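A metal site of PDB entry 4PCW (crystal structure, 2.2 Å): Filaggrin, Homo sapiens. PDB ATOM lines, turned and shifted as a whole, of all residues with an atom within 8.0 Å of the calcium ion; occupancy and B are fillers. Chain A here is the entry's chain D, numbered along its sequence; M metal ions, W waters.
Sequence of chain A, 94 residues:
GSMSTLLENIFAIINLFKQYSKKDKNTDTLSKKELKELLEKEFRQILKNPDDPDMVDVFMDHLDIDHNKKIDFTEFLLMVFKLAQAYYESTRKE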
ATOM      1  N   PHE A  17      11.823  16.276 -34.547  1.00  0.00           N
ATOM      2  CA  PHE A  17      10.488  16.434 -33.996  1.00  0.00           C
ATOM      3  C   PHE A  17      10.071  15.190 -33.202  1.00  0.00           C
ATOM      4  O   PHE A  17       9.420  15.299 -32.161  1.00  0.00           O
ATOM      5  CB  PHE A  17       9.480  16.712 -35.118  1.00  0.00           C
ATOM      6  CG  PHE A  17       8.056  16.787 -34.652  1.00  0.00           C
ATOM      7  CD1 PHE A  17       7.511  17.979 -34.212  1.00  0.00           C
ATOM      8  CD2 PHE A  17       7.262  15.654 -34.658  1.00  0.00           C
ATOM      9  CE1 PHE A  17       6.200  18.037 -33.786  1.00  0.00           C
ATOM     10  CE2 PHE A  17       5.951  15.711 -34.232  1.00  0.00           C
ATOM     11  CZ  PHE A  17       5.422  16.906 -33.798  1.00  0.00           C
ATOM     12  N   LYS A  18      10.449  14.023 -33.705  1.00  0.00           N
ATOM     13  CA  LYS A  18      10.070  12.760 -33.092  1.00  0.00           C
ATOM     14  C   LYS A  18      10.723  12.557 -31.726  1.00  0.00           C
ATOM     15  O   LYS A  18      10.084  12.041 -30.807  1.00  0.00           O
ATOM     16  CB  LYS A  18      10.434  11.579 -34.005  1.00  0.00           C
ATOM     17  CG  LYS A  18       9.316  11.163 -34.946  1.00  0.00           C
ATOM     18  CD  LYS A  18       9.714   9.920 -35.734  1.00  0.00           C
ATOM     19  CE  LYS A  18       8.607   9.491 -36.687  1.00  0.00           C
ATOM     20  NZ  LYS A  18       7.322   9.231 -35.979  1.00  0.00           N
ATOM     21  N   TYR A  20      11.568  14.712 -29.564  1.00  0.00           N
ATOM     22  CA  TYR A  20      10.981  15.598 -28.563  1.00  0.00           C
ATOM     23  C   TYR A  20       9.528  15.244 -28.289  1.00  0.00           C
ATOM     24  O   TYR A  20       9.084  15.290 -27.147  1.00  0.00           O
ATOM     25  CB  TYR A  20      11.099  17.052 -29.007  1.00  0.00           C
ATOM     26  CG  TYR A  20      12.496  17.610 -28.876  1.00  0.00           C
ATOM     27  CD1 TYR A  20      12.962  18.119 -27.669  1.00  0.00           C
ATOM     28  CD2 TYR A  20      13.363  17.614 -29.957  1.00  0.00           C
ATOM     29  CE1 TYR A  20      14.239  18.623 -27.547  1.00  0.00           C
ATOM     30  CE2 TYR A  20      14.648  18.120 -29.846  1.00  0.00           C
ATOM     31  CZ  TYR A  20      15.078  18.616 -28.638  1.00  0.00           C
ATOM     32  OH  TYR A  20      16.351  19.112 -28.545  1.00  0.00           O
ATOM     33  N   SER A  21       8.784  14.903 -29.334  1.00  0.00           N
ATOM     34  CA  SER A  21       7.361  14.620 -29.193  1.00  0.00           C
ATOM     35  C   SER A  21       7.120  13.326 -28.435  1.00  0.00           C
ATOM     36  O   SER A  21       6.114  13.180 -27.733  1.00  0.00           O
ATOM     37  CB  SER A  21       6.691  14.563 -30.569  1.00  0.00           C
ATOM     38  OG  SER A  21       7.205  13.503 -31.352  1.00  0.00           O
ATOM     39  N   LYS A  22       8.054  12.379 -28.548  1.00  0.00           N
ATOM     40  CA  LYS A  22       7.878  11.056 -27.972  1.00  0.00           C
ATOM     41  C   LYS A  22       8.200  10.984 -26.482  1.00  0.00           C
ATOM     42  O   LYS A  22       8.117   9.918 -25.881  1.00  0.00           O
ATOM     43  CB  LYS A  22       8.742  10.035 -28.726  1.00  0.00           C
ATOM     44  CG  LYS A  22       8.160   9.612 -30.066  1.00  0.00           C
ATOM     45  CD  LYS A  22       8.936   8.444 -30.657  1.00  0.00           C
ATOM     46  CE  LYS A  22       8.239   7.871 -31.887  1.00  0.00           C
ATOM     47  NZ  LYS A  22       8.905   6.641 -32.372  1.00  0.00           N
ATOM     48  N   LYS A  23       8.562  12.114 -25.883  1.00  0.00           N
ATOM     49  CA  LYS A  23       8.824  12.149 -24.453  1.00  0.00           C
ATOM     50  C   LYS A  23       7.515  11.976 -23.690  1.00  0.00           C
ATOM     51  O   LYS A  23       7.469  11.314 -22.649  1.00  0.00           O
ATOM     52  CB  LYS A  23       9.500  13.461 -24.035  1.00  0.00           C
ATOM     53  CG  LYS A  23      10.673  13.879 -24.899  1.00  0.00           C
ATOM     54  CD  LYS A  23      11.994  13.960 -24.139  1.00  0.00           C
ATOM     55  CE  LYS A  23      12.707  15.266 -24.427  1.00  0.00           C
ATOM     56  NZ  LYS A  23      14.064  15.320 -23.842  1.00  0.00           N
ATOM     57  N   ASP A  24       6.455  12.568 -24.220  1.00  0.00           N
ATOM     58  CA  ASP A  24       5.126  12.461 -23.623  1.00  0.00           C
ATOM     59  C   ASP A  24       4.430  11.174 -24.017  1.00  0.00           C
ATOM     60  O   ASP A  24       4.929  10.391 -24.817  1.00  0.00           O
ATOM     61  CB  ASP A  24       4.265  13.654 -24.033  1.00  0.00           C
ATOM     62  CG  ASP A  24       4.492  14.879 -23.180  1.00  0.00           C
ATOM     63  OD1 ASP A  24       5.613  15.055 -22.665  1.00  0.00           O
ATOM     64  OD2 ASP A  24       3.538  15.671 -23.023  1.00  0.00           O
ATOM     65  N   LYS A  25       3.256  10.977 -23.432  1.00  0.00           N
ATOM     66  CA  LYS A  25       2.376   9.875 -23.787  1.00  0.00           C
ATOM     67  C   LYS A  25       1.741  10.146 -25.158  1.00  0.00           C
ATOM     68  O   LYS A  25       1.392   9.221 -25.892  1.00  0.00           O
ATOM     69  CB  LYS A  25       1.310   9.711 -22.702  1.00  0.00           C
ATOM     70  CG  LYS A  25       0.056   8.960 -23.096  1.00  0.00           C
ATOM     71  CD  LYS A  25      -0.879   8.828 -21.905  1.00  0.00           C
ATOM     72  CE  LYS A  25      -1.391  10.183 -21.423  1.00  0.00           C
ATOM     73  NZ  LYS A  25      -2.437  10.051 -20.373  1.00  0.00           N
ATOM     74  N   ASN A  26       1.600  11.427 -25.488  1.00  0.00           N
ATOM     75  CA  ASN A  26       1.175  11.845 -26.823  1.00  0.00           C
ATOM     76  C   ASN A  26       2.377  11.933 -27.752  1.00  0.00           C
ATOM     77  O   ASN A  26       3.032  12.967 -27.824  1.00  0.00           O
ATOM     78  CB  ASN A  26       0.446  13.190 -26.755  1.00  0.00           C
ATOM     79  CG  ASN A  26      -0.709  13.179 -25.786  1.00  0.00           C
ATOM     80  OD1 ASN A  26      -0.563  13.532 -24.612  1.00  0.00           O
ATOM     81  ND2 ASN A  26      -1.885  12.779 -26.263  1.00  0.00           N
ATOM     82  N   THR A  27       2.650  10.847 -28.458  1.00  0.00           N
ATOM     83  CA  THR A  27       3.873  10.720 -29.247  1.00  0.00           C
ATOM     84  C   THR A  27       3.868  11.588 -30.507  1.00  0.00           C
ATOM     85  O   THR A  27       4.911  11.893 -31.062  1.00  0.00           O
ATOM     86  CB  THR A  27       4.121   9.266 -29.658  1.00  0.00           C
ATOM     87  OG1 THR A  27       3.117   8.845 -30.586  1.00  0.00           O
ATOM     88  CG2 THR A  27       4.104   8.346 -28.445  1.00  0.00           C
ATOM     89  N   ASP A  28       2.676  11.985 -30.945  1.00  0.00           N
ATOM     90  CA  ASP A  28       2.510  12.656 -32.232  1.00  0.00           C
ATOM     91  C   ASP A  28       2.652  14.172 -32.144  1.00  0.00           C
ATOM     92  O   ASP A  28       2.653  14.856 -33.177  1.00  0.00           O
ATOM     93  CB  ASP A  28       1.150  12.301 -32.822  1.00  0.00           C
ATOM     94  CG  ASP A  28      -0.009  12.722 -31.937  1.00  0.00           C
ATOM     95  OD1 ASP A  28       0.147  12.659 -30.690  1.00  0.00           O
ATOM     96  OD2 ASP A  28      -1.065  13.107 -32.466  1.00  0.00           O
ATOM     97  N   THR A  29       2.758  14.711 -30.930  1.00  0.00           N
ATOM     98  CA  THR A  29       2.764  16.160 -30.735  1.00  0.00           C
ATOM     99  C   THR A  29       3.785  16.631 -29.698  1.00  0.00           C
ATOM    100  O   THR A  29       4.293  15.839 -28.898  1.00  0.00           O
ATOM    101  CB  THR A  29       1.376  16.663 -30.286  1.00  0.00           C
ATOM    102  OG1 THR A  29       0.952  15.932 -29.136  1.00  0.00           O
ATOM    103  CG2 THR A  29       0.360  16.489 -31.410  1.00  0.00           C
ATOM    104  N   LEU A  30       4.073  17.929 -29.729  1.00  0.00           N
ATOM    105  CA  LEU A  30       4.940  18.555 -28.730  1.00  0.00           C
ATOM    106  C   LEU A  30       4.102  19.258 -27.677  1.00  0.00           C
ATOM    107  O   LEU A  30       3.258  20.094 -28.002  1.00  0.00           O
ATOM    108  CB  LEU A  30       5.881  19.570 -29.389  1.00  0.00           C
ATOM    109  CG  LEU A  30       6.832  19.042 -30.466  1.00  0.00           C
ATOM    110  CD1 LEU A  30       7.438  20.222 -31.221  1.00  0.00           C
ATOM    111  CD2 LEU A  30       7.914  18.166 -29.855  1.00  0.00           C
ATOM    112  N   SER A  31       4.345  18.929 -26.414  1.00  0.00           N
ATOM    113  CA  SER A  31       3.726  19.643 -25.311  1.00  0.00           C
ATOM    114  C   SER A  31       4.426  20.987 -25.153  1.00  0.00           C
ATOM    115  O   SER A  31       5.382  21.282 -25.867  1.00  0.00           O
ATOM    116  CB  SER A  31       3.809  18.837 -24.017  1.00  0.00           C
ATOM    117  OG  SER A  31       5.156  18.630 -23.634  1.00  0.00           O
ATOM    118  N   LYS A  32       3.946  21.806 -24.226  1.00  0.00           N
ATOM    119  CA  LYS A  32       4.591  23.074 -23.952  1.00  0.00           C
ATOM    120  C   LYS A  32       5.973  22.838 -23.362  1.00  0.00           C
ATOM    121  O   LYS A  32       6.915  23.579 -23.640  1.00  0.00           O
ATOM    122  CB  LYS A  32       3.727  23.918 -22.999  1.00  0.00           C
ATOM    123  CG  LYS A  32       4.086  25.398 -22.995  1.00  0.00           C
ATOM    124  CD  LYS A  32       2.939  26.237 -22.432  1.00  0.00           C
ATOM    125  CE  LYS A  32       3.236  27.724 -22.535  1.00  0.00           C
ATOM    126  NZ  LYS A  32       4.423  28.119 -21.730  1.00  0.00           N
ATOM    127  N   GLU A  34       7.829  20.041 -23.905  1.00  0.00           N
ATOM    128  CA  GLU A  34       8.649  19.450 -24.955  1.00  0.00           C
ATOM    129  C   GLU A  34       9.131  20.508 -25.934  1.00  0.00           C
ATOM    130  O   GLU A  34      10.294  20.499 -26.366  1.00  0.00           O
ATOM    131  CB  GLU A  34       7.877  18.352 -25.690  1.00  0.00           C
ATOM    132  CG  GLU A  34       7.652  17.095 -24.874  1.00  0.00           C
ATOM    133  CD  GLU A  34       6.684  16.129 -25.524  1.00  0.00           C
ATOM    134  OE1 GLU A  34       5.799  16.589 -26.271  1.00  0.00           O
ATOM    135  OE2 GLU A  34       6.812  14.905 -25.297  1.00  0.00           O
ATOM    136  N   LEU A  35       8.236  21.429 -26.290  1.00  0.00           N
ATOM    137  CA  LEU A  35       8.577  22.541 -27.159  1.00  0.00           C
ATOM    138  C   LEU A  35       9.654  23.417 -26.526  1.00  0.00           C
ATOM    139  O   LEU A  35      10.570  23.877 -27.195  1.00  0.00           O
ATOM    140  CB  LEU A  35       7.329  23.371 -27.477  1.00  0.00           C
ATOM    141  CG  LEU A  35       7.515  24.631 -28.326  1.00  0.00           C
ATOM    142  CD1 LEU A  35       8.033  24.272 -29.714  1.00  0.00           C
ATOM    143  CD2 LEU A  35       6.214  25.397 -28.423  1.00  0.00           C
ATOM    144  N   LYS A  70      -1.057  22.050 -28.096  1.00  0.00           N
ATOM    145  CA  LYS A  70      -0.026  21.112 -28.519  1.00  0.00           C
ATOM    146  C   LYS A  70       0.407  21.443 -29.943  1.00  0.00           C
ATOM    147  O   LYS A  70      -0.347  22.045 -30.697  1.00  0.00           O
ATOM    148  CB  LYS A  70      -0.533  19.670 -28.419  1.00  0.00           C
ATOM    149  CG  LYS A  70      -0.803  19.214 -26.997  1.00  0.00           C
ATOM    150  CD  LYS A  70      -0.865  17.706 -26.880  1.00  0.00           C
ATOM    151  CE  LYS A  70      -2.185  17.147 -27.360  1.00  0.00           C
ATOM    152  NZ  LYS A  70      -3.295  17.473 -26.420  1.00  0.00           N
ATOM    153  N   ILE A  71       1.634  21.063 -30.286  1.00  0.00           N
ATOM    154  CA  ILE A  71       2.196  21.361 -31.605  1.00  0.00           C
ATOM    155  C   ILE A  71       2.410  20.097 -32.422  1.00  0.00           C
ATOM    156  O   ILE A  71       3.353  19.351 -32.174  1.00  0.00           O
ATOM    157  CB  ILE A  71       3.537  22.112 -31.486  1.00  0.00           C
ATOM    158  CG1 ILE A  71       3.403  23.313 -30.540  1.00  0.00           C
ATOM    159  CG2 ILE A  71       4.027  22.543 -32.852  1.00  0.00           C
ATOM    160  CD1 ILE A  71       2.410  24.365 -30.995  1.00  0.00           C
HETATM  161 CA    CA M   1       4.339  14.784 -26.736  1.00  0.00          CA
HETATM  162  O   HOH W   1       2.356  16.125 -26.314  1.00  0.00           O
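CB of Asp 24 touches the calcium ion, 2.9 Å away.
The calcium ion is bound by the side-chain carboxylate (OE1) of Glu 34, the backbone carbonyl oxygen (O) of Thr 29, water W1, the backbone carbonyl oxygen (O) of Asn 26, the backbone carbonyl oxygen (O) of Ser 21 and the side-chain carboxylate (OE2) of Glu 34.
Water W1 lies within hydrogen-bond range of OG1 of Thr 29 (3.2 Å) and N of Ser 31 (3.4 Å).
The backbone NH of Glu 34 is in hydrogen-bond range of the side-chain hydroxyl of Ser 31 (3.0 Å).
OE2 of Glu 34 lies close to N of Asp 24 (2.6 Å).
N of Lys 23 sits close to OE2 of Glu 34, at 3.3 Å.
The backbone carbonyl oxygen (O) of Thr 27 sits at hydrogen-bond distance from the side-chain hydroxyl (OG) of Ser 21, 2.8 Å away.
The side-chain hydroxyl of Ser 21 lies within hydrogen-bond range of the backbone carbonyl oxygen of Lys 18 (3.3 Å).
OG of Ser 21 lies within hydrogen-bond range of O of Phe 17.
The side-chain carboxylate (OD2) of Asp 24 sits close to the side-chain hydroxyl (OG) of Ser 31, at 3.4 Å.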
